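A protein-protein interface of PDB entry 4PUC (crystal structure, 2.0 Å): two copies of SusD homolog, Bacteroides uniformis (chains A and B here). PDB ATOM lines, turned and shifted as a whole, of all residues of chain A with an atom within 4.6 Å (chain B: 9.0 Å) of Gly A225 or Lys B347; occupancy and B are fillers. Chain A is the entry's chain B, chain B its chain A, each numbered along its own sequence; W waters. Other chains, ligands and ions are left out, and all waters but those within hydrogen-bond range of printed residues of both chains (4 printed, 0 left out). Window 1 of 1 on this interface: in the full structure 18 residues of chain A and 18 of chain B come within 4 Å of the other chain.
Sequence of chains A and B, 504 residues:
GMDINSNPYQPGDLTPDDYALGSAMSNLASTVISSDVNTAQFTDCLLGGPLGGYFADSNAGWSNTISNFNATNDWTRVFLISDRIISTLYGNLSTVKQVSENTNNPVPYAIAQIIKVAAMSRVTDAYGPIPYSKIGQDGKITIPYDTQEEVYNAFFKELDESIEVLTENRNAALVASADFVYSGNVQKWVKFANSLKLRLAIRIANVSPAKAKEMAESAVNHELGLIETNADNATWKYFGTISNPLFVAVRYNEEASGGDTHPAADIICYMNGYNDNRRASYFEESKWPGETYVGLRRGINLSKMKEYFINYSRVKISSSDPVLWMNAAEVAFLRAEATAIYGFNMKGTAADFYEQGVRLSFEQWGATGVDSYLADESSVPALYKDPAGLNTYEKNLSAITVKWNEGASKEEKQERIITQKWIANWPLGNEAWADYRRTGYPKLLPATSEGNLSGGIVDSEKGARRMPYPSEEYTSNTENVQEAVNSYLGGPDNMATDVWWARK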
ATOM      1  N   VAL A 190      12.779  13.631 -29.656  1.00  0.00           N
ATOM      2  CA  VAL A 190      11.482  14.203 -29.300  1.00  0.00           C
ATOM      3  C   VAL A 190      11.566  15.727 -29.138  1.00  0.00           C
ATOM      4  O   VAL A 190      10.678  16.443 -29.602  1.00  0.00           O
ATOM      5  CB  VAL A 190      10.905  13.593 -28.013  1.00  0.00           C
ATOM      6  CG1 VAL A 190       9.667  14.355 -27.569  1.00  0.00           C
ATOM      7  CG2 VAL A 190      10.568  12.126 -28.230  1.00  0.00           C
ATOM      8  N   LYS A 191      12.618  16.210 -28.478  1.00  0.00           N
ATOM      9  CA  LYS A 191      12.811  17.653 -28.296  1.00  0.00           C
ATOM     10  C   LYS A 191      12.898  18.387 -29.623  1.00  0.00           C
ATOM     11  O   LYS A 191      12.338  19.473 -29.777  1.00  0.00           O
ATOM     12  CB  LYS A 191      14.071  17.943 -27.484  1.00  0.00           C
ATOM     13  CG  LYS A 191      13.928  17.634 -26.008  1.00  0.00           C
ATOM     14  CD  LYS A 191      15.202  17.941 -25.241  1.00  0.00           C
ATOM     15  CE  LYS A 191      14.940  18.005 -23.752  1.00  0.00           C
ATOM     16  NZ  LYS A 191      14.057  19.164 -23.408  1.00  0.00           N
ATOM     17  N   ASN A 194       9.318  18.420 -31.230  1.00  0.00           N
ATOM     18  CA  ASN A 194       8.517  19.504 -30.635  1.00  0.00           C
ATOM     19  C   ASN A 194       8.981  20.881 -31.087  1.00  0.00           C
ATOM     20  O   ASN A 194       8.164  21.797 -31.265  1.00  0.00           O
ATOM     21  CB  ASN A 194       8.556  19.468 -29.104  1.00  0.00           C
ATOM     22  CG  ASN A 194       7.823  18.281 -28.516  1.00  0.00           C
ATOM     23  OD1 ASN A 194       6.768  17.878 -29.004  1.00  0.00           O
ATOM     24  ND2 ASN A 194       8.385  17.715 -27.455  1.00  0.00           N
ATOM     25  N   VAL A 220       4.882  23.100 -26.589  1.00  0.00           N
ATOM     26  CA  VAL A 220       5.424  23.532 -25.295  1.00  0.00           C
ATOM     27  C   VAL A 220       4.779  22.827 -24.097  1.00  0.00           C
ATOM     28  O   VAL A 220       5.319  22.883 -23.000  1.00  0.00           O
ATOM     29  CB  VAL A 220       5.317  25.061 -25.073  1.00  0.00           C
ATOM     30  CG1 VAL A 220       6.115  25.804 -26.121  1.00  0.00           C
ATOM     31  CG2 VAL A 220       3.878  25.525 -25.082  1.00  0.00           C
ATOM     32  N   ASN A 221       3.634  22.179 -24.293  1.00  0.00           N
ATOM     33  CA  ASN A 221       3.009  21.408 -23.222  1.00  0.00           C
ATOM     34  C   ASN A 221       3.565  20.005 -23.047  1.00  0.00           C
ATOM     35  O   ASN A 221       3.251  19.347 -22.063  1.00  0.00           O
ATOM     36  CB  ASN A 221       1.500  21.339 -23.414  1.00  0.00           C
ATOM     37  CG  ASN A 221       0.782  22.372 -22.589  1.00  0.00           C
ATOM     38  OD1 ASN A 221       0.776  22.291 -21.354  1.00  0.00           O
ATOM     39  ND2 ASN A 221       0.208  23.376 -23.252  1.00  0.00           N
ATOM     40  N   HIS A 222       4.382  19.554 -23.995  1.00  0.00           N
ATOM     41  CA  HIS A 222       4.808  18.175 -24.019  1.00  0.00           C
ATOM     42  C   HIS A 222       5.776  17.878 -22.879  1.00  0.00           C
ATOM     43  O   HIS A 222       6.618  18.701 -22.529  1.00  0.00           O
ATOM     44  CB  HIS A 222       5.441  17.813 -25.361  1.00  0.00           C
ATOM     45  CG  HIS A 222       5.646  16.345 -25.525  1.00  0.00           C
ATOM     46  ND1 HIS A 222       6.832  15.722 -25.204  1.00  0.00           N
ATOM     47  CD2 HIS A 222       4.791  15.365 -25.905  1.00  0.00           C
ATOM     48  CE1 HIS A 222       6.712  14.425 -25.416  1.00  0.00           C
ATOM     49  NE2 HIS A 222       5.483  14.182 -25.836  1.00  0.00           N
ATOM     50  N   GLU A 223       5.638  16.700 -22.289  1.00  0.00           N
ATOM     51  CA  GLU A 223       6.402  16.362 -21.087  1.00  0.00           C
ATOM     52  C   GLU A 223       7.924  16.366 -21.235  1.00  0.00           C
ATOM     53  O   GLU A 223       8.622  16.513 -20.245  1.00  0.00           O
ATOM     54  CB  GLU A 223       5.951  15.013 -20.524  1.00  0.00           C
ATOM     55  CG  GLU A 223       6.127  13.837 -21.469  1.00  0.00           C
ATOM     56  CD  GLU A 223       5.557  12.561 -20.891  1.00  0.00           C
ATOM     57  OE1 GLU A 223       6.164  12.032 -19.943  1.00  0.00           O
ATOM     58  OE2 GLU A 223       4.496  12.099 -21.375  1.00  0.00           O
ATOM     59  N   LEU A 224       8.436  16.201 -22.455  1.00  0.00           N
ATOM     60  CA  LEU A 224       9.886  16.159 -22.680  1.00  0.00           C
ATOM     61  C   LEU A 224      10.465  17.488 -23.158  1.00  0.00           C
ATOM     62  O   LEU A 224      11.683  17.641 -23.271  1.00  0.00           O
ATOM     63  CB  LEU A 224      10.242  15.037 -23.654  1.00  0.00           C
ATOM     64  CG  LEU A 224      10.061  13.621 -23.102  1.00  0.00           C
ATOM     65  CD1 LEU A 224      10.334  12.570 -24.170  1.00  0.00           C
ATOM     66  CD2 LEU A 224      10.951  13.397 -21.875  1.00  0.00           C
ATOM     67  N   GLY A 225       9.598  18.457 -23.431  1.00  0.00           N
ATOM     68  CA  GLY A 225      10.069  19.797 -23.727  1.00  0.00           C
ATOM     69  C   GLY A 225      10.686  19.950 -25.103  1.00  0.00           C
ATOM     70  O   GLY A 225      10.588  19.067 -25.963  1.00  0.00           O
ATOM     71  N   LEU A 226      11.319  21.098 -25.300  1.00  0.00           N
ATOM     72  CA  LEU A 226      11.923  21.451 -26.564  1.00  0.00           C
ATOM     73  C   LEU A 226      13.435  21.514 -26.427  1.00  0.00           C
ATOM     74  O   LEU A 226      13.977  21.195 -25.374  1.00  0.00           O
ATOM     75  CB  LEU A 226      11.354  22.783 -27.027  1.00  0.00           C
ATOM     76  CG  LEU A 226       9.849  22.730 -27.321  1.00  0.00           C
ATOM     77  CD1 LEU A 226       9.051  23.173 -26.112  1.00  0.00           C
ATOM     78  CD2 LEU A 226       9.483  23.614 -28.498  1.00  0.00           C
ATOM     79  N   LYS A 347       3.817  29.557 -21.243  1.00  0.00           N
ATOM     80  CA  LYS A 347       4.273  29.285 -19.867  1.00  0.00           C
ATOM     81  C   LYS A 347       5.510  30.085 -19.473  1.00  0.00           C
ATOM     82  O   LYS A 347       6.447  29.580 -18.848  1.00  0.00           O
ATOM     83  CB  LYS A 347       4.478  27.789 -19.672  1.00  0.00           C
ATOM     84  CG  LYS A 347       3.182  27.026 -19.854  1.00  0.00           C
ATOM     85  CD  LYS A 347       3.343  25.791 -20.704  1.00  0.00           C
ATOM     86  CE  LYS A 347       2.223  24.799 -20.449  1.00  0.00           C
ATOM     87  NZ  LYS A 347       0.839  25.350 -20.284  1.00  0.00           N
ATOM     88  N   ALA B 216       3.494  20.812  -7.818  1.00  0.00           N
ATOM     89  CA  ALA B 216       4.665  20.974  -8.679  1.00  0.00           C
ATOM     90  C   ALA B 216       4.272  21.164 -10.154  1.00  0.00           C
ATOM     91  O   ALA B 216       4.747  22.089 -10.820  1.00  0.00           O
ATOM     92  CB  ALA B 216       5.607  19.784  -8.527  1.00  0.00           C
ATOM     93  N   GLU B 217       3.413  20.283 -10.661  1.00  0.00           N
ATOM     94  CA  GLU B 217       3.061  20.299 -12.079  1.00  0.00           C
ATOM     95  C   GLU B 217       2.197  21.508 -12.388  1.00  0.00           C
ATOM     96  O   GLU B 217       2.335  22.122 -13.441  1.00  0.00           O
ATOM     97  CB  GLU B 217       2.395  18.982 -12.504  1.00  0.00           C
ATOM     98  CG  GLU B 217       3.367  17.798 -12.512  1.00  0.00           C
ATOM     99  CD  GLU B 217       2.730  16.462 -12.873  1.00  0.00           C
ATOM    100  OE1 GLU B 217       1.505  16.397 -13.068  1.00  0.00           O
ATOM    101  OE2 GLU B 217       3.462  15.453 -12.953  1.00  0.00           O
ATOM    102  N   SER B 218       1.328  21.872 -11.454  1.00  0.00           N
ATOM    103  CA  SER B 218       0.510  23.082 -11.590  1.00  0.00           C
ATOM    104  C   SER B 218       1.370  24.344 -11.694  1.00  0.00           C
ATOM    105  O   SER B 218       1.099  25.224 -12.505  1.00  0.00           O
ATOM    106  CB  SER B 218      -0.414  23.209 -10.386  1.00  0.00           C
ATOM    107  OG  SER B 218      -1.073  24.453 -10.381  1.00  0.00           O
ATOM    108  N   ALA B 219       2.411  24.427 -10.870  1.00  0.00           N
ATOM    109  CA  ALA B 219       3.299  25.578 -10.886  1.00  0.00           C
ATOM    110  C   ALA B 219       3.939  25.771 -12.260  1.00  0.00           C
ATOM    111  O   ALA B 219       3.875  26.860 -12.831  1.00  0.00           O
ATOM    112  CB  ALA B 219       4.380  25.418  -9.829  1.00  0.00           C
ATOM    113  N   VAL B 220       4.519  24.692 -12.787  1.00  0.00           N
ATOM    114  CA  VAL B 220       5.192  24.702 -14.086  1.00  0.00           C
ATOM    115  C   VAL B 220       4.250  24.914 -15.290  1.00  0.00           C
ATOM    116  O   VAL B 220       4.681  25.346 -16.369  1.00  0.00           O
ATOM    117  CB  VAL B 220       6.046  23.416 -14.260  1.00  0.00           C
ATOM    118  CG1 VAL B 220       5.208  22.228 -14.706  1.00  0.00           C
ATOM    119  CG2 VAL B 220       7.186  23.631 -15.234  1.00  0.00           C
ATOM    120  N   ASN B 221       2.972  24.610 -15.098  1.00  0.00           N
ATOM    121  CA  ASN B 221       1.990  24.757 -16.149  1.00  0.00           C
ATOM    122  C   ASN B 221       1.397  26.142 -16.279  1.00  0.00           C
ATOM    123  O   ASN B 221       0.699  26.418 -17.247  1.00  0.00           O
ATOM    124  CB  ASN B 221       0.863  23.751 -15.968  1.00  0.00           C
ATOM    125  CG  ASN B 221       1.078  22.524 -16.806  1.00  0.00           C
ATOM    126  OD1 ASN B 221       1.033  22.600 -18.035  1.00  0.00           O
ATOM    127  ND2 ASN B 221       1.349  21.396 -16.161  1.00  0.00           N
ATOM    128  N   HIS B 222       1.695  27.018 -15.328  1.00  0.00           N
ATOM    129  CA  HIS B 222       1.054  28.318 -15.296  1.00  0.00           C
ATOM    130  C   HIS B 222       1.535  29.189 -16.457  1.00  0.00           C
ATOM    131  O   HIS B 222       2.708  29.153 -16.827  1.00  0.00           O
ATOM    132  CB  HIS B 222       1.299  29.007 -13.956  1.00  0.00           C
ATOM    133  CG  HIS B 222       0.476  30.241 -13.777  1.00  0.00           C
ATOM    134  ND1 HIS B 222       0.957  31.495 -14.079  1.00  0.00           N
ATOM    135  CD2 HIS B 222      -0.811  30.412 -13.390  1.00  0.00           C
ATOM    136  CE1 HIS B 222       0.008  32.389 -13.872  1.00  0.00           C
ATOM    137  NE2 HIS B 222      -1.072  31.759 -13.441  1.00  0.00           N
ATOM    138  N   LEU B 226       7.894  30.362 -14.081  1.00  0.00           N
ATOM    139  CA  LEU B 226       8.608  30.500 -12.821  1.00  0.00           C
ATOM    140  C   LEU B 226       9.789  31.446 -12.971  1.00  0.00           C
ATOM    141  O   LEU B 226       9.966  32.052 -14.023  1.00  0.00           O
ATOM    142  CB  LEU B 226       9.104  29.130 -12.370  1.00  0.00           C
ATOM    143  CG  LEU B 226       7.950  28.171 -12.071  1.00  0.00           C
ATOM    144  CD1 LEU B 226       7.670  27.315 -13.284  1.00  0.00           C
ATOM    145  CD2 LEU B 226       8.276  27.277 -10.899  1.00  0.00           C
ATOM    146  N   GLU B 228      13.081  32.103 -14.012  1.00  0.00           N
ATOM    147  CA  GLU B 228      13.963  31.451 -14.970  1.00  0.00           C
ATOM    148  C   GLU B 228      15.234  32.219 -15.272  1.00  0.00           C
ATOM    149  O   GLU B 228      16.185  31.652 -15.807  1.00  0.00           O
ATOM    150  CB  GLU B 228      13.216  31.209 -16.267  1.00  0.00           C
ATOM    151  CG  GLU B 228      12.242  30.056 -16.163  1.00  0.00           C
ATOM    152  CD  GLU B 228      12.093  29.303 -17.452  1.00  0.00           C
ATOM    153  OE1 GLU B 228      12.282  29.918 -18.527  1.00  0.00           O
ATOM    154  OE2 GLU B 228      11.782  28.098 -17.383  1.00  0.00           O
ATOM    155  N   ARG B 335      13.149  21.483 -10.526  1.00  0.00           N
ATOM    156  CA  ARG B 335      12.622  20.783 -11.691  1.00  0.00           C
ATOM    157  C   ARG B 335      13.441  19.533 -12.003  1.00  0.00           C
ATOM    158  O   ARG B 335      12.886  18.505 -12.374  1.00  0.00           O
ATOM    159  CB  ARG B 335      12.559  21.721 -12.895  1.00  0.00           C
ATOM    160  CG  ARG B 335      11.537  22.828 -12.728  1.00  0.00           C
ATOM    161  CD  ARG B 335      11.475  23.744 -13.943  1.00  0.00           C
ATOM    162  NE  ARG B 335      12.573  24.697 -13.983  1.00  0.00           N
ATOM    163  CZ  ARG B 335      12.616  25.737 -14.807  1.00  0.00           C
ATOM    164  NH1 ARG B 335      11.628  25.940 -15.663  1.00  0.00           N
ATOM    165  NH2 ARG B 335      13.648  26.567 -14.779  1.00  0.00           N
ATOM    166  N   ALA B 338      12.342  17.041  -9.323  1.00  0.00           N
ATOM    167  CA  ALA B 338      10.964  16.694  -9.611  1.00  0.00           C
ATOM    168  C   ALA B 338      10.884  15.609 -10.691  1.00  0.00           C
ATOM    169  O   ALA B 338      10.144  14.632 -10.545  1.00  0.00           O
ATOM    170  CB  ALA B 338      10.164  17.938 -10.020  1.00  0.00           C
ATOM    171  N   THR B 339      11.627  15.792 -11.780  1.00  0.00           N
ATOM    172  CA  THR B 339      11.643  14.818 -12.878  1.00  0.00           C
ATOM    173  C   THR B 339      12.396  13.541 -12.522  1.00  0.00           C
ATOM    174  O   THR B 339      11.848  12.454 -12.637  1.00  0.00           O
ATOM    175  CB  THR B 339      12.306  15.390 -14.150  1.00  0.00           C
ATOM    176  OG1 THR B 339      13.246  16.411 -13.787  1.00  0.00           O
ATOM    177  CG2 THR B 339      11.264  15.969 -15.085  1.00  0.00           C
ATOM    178  N   PHE B 344       7.801  13.584 -11.883  1.00  0.00           N
ATOM    179  CA  PHE B 344       6.790  14.582 -12.254  1.00  0.00           C
ATOM    180  C   PHE B 344       7.051  15.104 -13.663  1.00  0.00           C
ATOM    181  O   PHE B 344       8.181  15.071 -14.156  1.00  0.00           O
ATOM    182  CB  PHE B 344       6.762  15.765 -11.270  1.00  0.00           C
ATOM    183  CG  PHE B 344       6.494  15.387  -9.833  1.00  0.00           C
ATOM    184  CD1 PHE B 344       5.865  14.192  -9.490  1.00  0.00           C
ATOM    185  CD2 PHE B 344       6.844  16.258  -8.814  1.00  0.00           C
ATOM    186  CE1 PHE B 344       5.631  13.874  -8.160  1.00  0.00           C
ATOM    187  CE2 PHE B 344       6.606  15.945  -7.482  1.00  0.00           C
ATOM    188  CZ  PHE B 344       5.999  14.753  -7.159  1.00  0.00           C
ATOM    189  N   ASN B 345       5.992  15.612 -14.293  1.00  0.00           N
ATOM    190  CA  ASN B 345       6.067  16.172 -15.636  1.00  0.00           C
ATOM    191  C   ASN B 345       6.459  17.656 -15.587  1.00  0.00           C
ATOM    192  O   ASN B 345       5.625  18.525 -15.321  1.00  0.00           O
ATOM    193  CB  ASN B 345       4.716  15.984 -16.327  1.00  0.00           C
ATOM    194  CG  ASN B 345       4.688  16.543 -17.735  1.00  0.00           C
ATOM    195  OD1 ASN B 345       5.610  17.235 -18.170  1.00  0.00           O
ATOM    196  ND2 ASN B 345       3.610  16.255 -18.450  1.00  0.00           N
ATOM    197  N   MET B 346       7.731  17.933 -15.849  1.00  0.00           N
ATOM    198  CA  MET B 346       8.274  19.291 -15.792  1.00  0.00           C
ATOM    199  C   MET B 346       8.540  19.901 -17.151  1.00  0.00           C
ATOM    200  O   MET B 346       9.271  20.884 -17.252  1.00  0.00           O
ATOM    201  CB  MET B 346       9.596  19.221 -15.035  1.00  0.00           C
ATOM    202  CG  MET B 346       9.450  18.810 -13.577  1.00  0.00           C
ATOM    203  SD  MET B 346       8.590  20.285 -12.574  1.00  0.00           S
ATOM    204  CE  MET B 346       6.873  19.446 -12.197  1.00  0.00           C
ATOM    205  N   LYS B 347       7.971  19.323 -18.209  1.00  0.00           N
ATOM    206  CA  LYS B 347       8.188  19.802 -19.578  1.00  0.00           C
ATOM    207  C   LYS B 347       9.661  19.895 -19.950  1.00  0.00           C
ATOM    208  O   LYS B 347      10.074  20.858 -20.605  1.00  0.00           O
ATOM    209  CB  LYS B 347       7.624  21.208 -19.786  1.00  0.00           C
ATOM    210  CG  LYS B 347       6.335  21.566 -19.074  1.00  0.00           C
ATOM    211  CD  LYS B 347       5.217  20.642 -19.465  1.00  0.00           C
ATOM    212  CE  LYS B 347       3.883  21.193 -18.998  1.00  0.00           C
ATOM    213  NZ  LYS B 347       2.861  20.173 -19.279  1.00  0.00           N
ATOM    214  N   GLY B 348      10.452  18.915 -19.536  1.00  0.00           N
ATOM    215  CA  GLY B 348      11.874  18.919 -19.834  1.00  0.00           C
ATOM    216  C   GLY B 348      12.558  17.752 -19.167  1.00  0.00           C
ATOM    217  O   GLY B 348      11.892  16.878 -18.607  1.00  0.00           O
ATOM    218  N   THR B 349      13.888  17.747 -19.233  1.00  0.00           N
ATOM    219  CA  THR B 349      14.687  16.619 -18.786  1.00  0.00           C
ATOM    220  C   THR B 349      15.610  17.021 -17.655  1.00  0.00           C
ATOM    221  O   THR B 349      16.066  18.166 -17.586  1.00  0.00           O
ATOM    222  CB  THR B 349      15.557  16.048 -19.928  1.00  0.00           C
ATOM    223  OG1 THR B 349      16.472  17.050 -20.403  1.00  0.00           O
ATOM    224  CG2 THR B 349      14.676  15.557 -21.061  1.00  0.00           C
ATOM    225  N   ALA B 350      15.892  16.060 -16.788  1.00  0.00           N
ATOM    226  CA  ALA B 350      16.751  16.290 -15.622  1.00  0.00           C
ATOM    227  C   ALA B 350      18.142  16.775 -16.005  1.00  0.00           C
ATOM    228  O   ALA B 350      18.693  17.670 -15.353  1.00  0.00           O
ATOM    229  CB  ALA B 350      16.870  15.022 -14.805  1.00  0.00           C
ATOM    230  N   ASP B 352      19.064  18.546 -18.520  1.00  0.00           N
ATOM    231  CA  ASP B 352      18.986  19.957 -18.883  1.00  0.00           C
ATOM    232  C   ASP B 352      18.852  20.830 -17.640  1.00  0.00           C
ATOM    233  O   ASP B 352      19.578  21.810 -17.480  1.00  0.00           O
ATOM    234  CB  ASP B 352      17.803  20.226 -19.828  1.00  0.00           C
ATOM    235  CG  ASP B 352      18.006  19.638 -21.220  1.00  0.00           C
ATOM    236  OD1 ASP B 352      19.035  18.973 -21.473  1.00  0.00           O
ATOM    237  OD2 ASP B 352      17.127  19.856 -22.077  1.00  0.00           O
ATOM    238  N   PHE B 353      17.918  20.466 -16.766  1.00  0.00           N
ATOM    239  CA  PHE B 353      17.631  21.262 -15.586  1.00  0.00           C
ATOM    240  C   PHE B 353      18.846  21.365 -14.661  1.00  0.00           C
ATOM    241  O   PHE B 353      19.139  22.445 -14.144  1.00  0.00           O
ATOM    242  CB  PHE B 353      16.420  20.699 -14.838  1.00  0.00           C
ATOM    243  CG  PHE B 353      15.116  20.842 -15.583  1.00  0.00           C
ATOM    244  CD1 PHE B 353      14.756  22.056 -16.165  1.00  0.00           C
ATOM    245  CD2 PHE B 353      14.231  19.769 -15.691  1.00  0.00           C
ATOM    246  CE1 PHE B 353      13.557  22.199 -16.855  1.00  0.00           C
ATOM    247  CE2 PHE B 353      13.023  19.914 -16.384  1.00  0.00           C
ATOM    248  CZ  PHE B 353      12.694  21.134 -16.957  1.00  0.00           C
ATOM    249  N   GLN B 356      21.349  23.729 -16.424  1.00  0.00           N
ATOM    250  CA  GLN B 356      20.804  25.083 -16.372  1.00  0.00           C
ATOM    251  C   GLN B 356      20.960  25.720 -14.988  1.00  0.00           C
ATOM    252  O   GLN B 356      21.251  26.904 -14.874  1.00  0.00           O
ATOM    253  CB  GLN B 356      19.321  25.112 -16.807  1.00  0.00           C
ATOM    254  CG  GLN B 356      19.133  24.819 -18.282  1.00  0.00           C
ATOM    255  CD  GLN B 356      17.670  24.657 -18.691  1.00  0.00           C
ATOM    256  OE1 GLN B 356      16.879  23.986 -18.015  1.00  0.00           O
ATOM    257  NE2 GLN B 356      17.312  25.261 -19.814  1.00  0.00           N
HETATM  258  O   HOH W   1       7.004  27.122 -17.176  1.00  0.00           O
HETATM  259  O   HOH W   2       2.596  16.832 -20.835  1.00  0.00           O
HETATM  260  O   HOH W   3      14.739  20.073 -20.745  1.00  0.00           O
HETATM  261  O   HOH W   4      -1.184  21.419 -18.973  1.00  0.00           O
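Lys A191 touches Thr B349. Lys B347 touches His A222 (CA to O, 3.5 Å). Glu A223 touches Asn B345. Lys B347 touches Glu A223. Leu A224 touches Gly B348. Gly A225 touches Lys B347 (CA to O, 3.3 Å). His B222 touches Lys A347 (O to CA, 3.4 Å).
Asn A221 touches its own counterpart, Asn B221. Asn A221 touches Lys B347, and with the chains exchanged Lys A347 touches Asn B221. His A222 touches Lys B347, and with the chains exchanged Lys A347 touches His B222. Positions printed for both chains: 220, 221, 222, 226 and 347.
Of the 22 printed residues of chain B, 7 touch a printed residue of chain A. Of the 11 printed residues of chain A, 7 touch a printed residue of chain B. Along chain A the printed residues that touch a printed residue of chain B span positions 191 to 347. Among the printed residues, Asp or Glu carboxylates within 4 Å of a Lys or Arg side-chain nitrogen of the other chain: Lys A191 with Asp B352.
Water W2 lies within hydrogen-bond range of the side-chain amide nitrogen of Asn B345 (2.7 Å), the backbone carbonyl oxygen of Asn A221 (2.9 Å) and the backbone NH of Glu A223 (3.4 Å). Water W4 bridges OD1 of Asn B221 (2.7 Å) and OD1 of Asn A221 (3.2 Å). Water W3 lies within hydrogen-bond range of the side-chain carboxylate (OD2) of Asp B352 (2.7 Å), the side-chain amino group (NZ) of Lys A191 (2.9 Å) and the backbone NH (N) of Thr B349 (2.9 Å). Water W1 lies within hydrogen-bond range of O of Lys A347 (3.0 Å) and O of Val B220 (3.0 Å).
The side-chain carboxylate (OD2) of Asp B352 is in salt-bridge range of the side-chain amino group (NZ) of Lys A191, 3.4 Å away. The side-chain amino group (NZ) of Lys B347 is in hydrogen-bond range of the backbone carbonyl oxygen (O) of Asn A221 (2.9 Å). OD1 of Asn A221 sits close to OD1 of Asn B221, 3.3 Å away. The backbone carbonyl oxygen (O) of Glu A223 sits at hydrogen-bond distance from the backbone NH (N) of Gly B348, 3.1 Å away. The side-chain amino group of Lys A347 lies within hydrogen-bond range of the backbone carbonyl oxygen of Asn B221 (3.2 Å).
OD1 of Asn A221 sits close to NZ of Lys A347, at 3.2 Å. The side-chain carboxylate (OD2) of Asp B352 lies close to the side-chain hydroxyl (OG1) of Thr B349 (3.3 Å). NZ of Lys A191 is in hydrogen-bond range of O of Leu A226 (2.8 Å). The side-chain carboxylate (OE2) of Glu B217 lies within hydrogen-bond range of the backbone NH (N) of Asn B345. The backbone NH (N) of Leu A224 sits close to a ring nitrogen (ND1) of His A222 (3.2 Å). NZ of Lys B347 is in hydrogen-bond range of OD1 of Asn B221 (3.3 Å).
Lys A191 touches just these residues of chain B: Thr B349 and Asp B352. Printed residues of chain B within 4 Å of Asn A221: Asn B221 and Lys B347. Of the printed residues of chain B, His A222 touches Lys B347. Of the printed residues of chain B, Leu A224 touches Gly B348. Printed residues of chain B within 4 Å of Gly A225: Lys B347. Val B220 touches none of the printed residues of chain A. Of the printed residues of chain A, His B222 touches Lys A347 (3.4 Å). Glu B228 touches none of the printed residues of chain A. Printed residues of chain A within 4 Å of Lys B347: Asn A221 (2.9 Å), His A222 (3.5 Å), Glu A223 (3.4 Å) and Gly A225 (3.3 Å). Of the printed residues of chain A, Thr B349 touches Lys A191. The nearest printed residue of chain B that does not touch Gly A225 is Gly B348 (4.01 Å). The nearest residue of chain A that does not touch Lys B347 is Leu A224 (4.1 Å). The nearest printed residue of chain B that does not touch Asn A221 is Asn B345 (4.8 Å).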
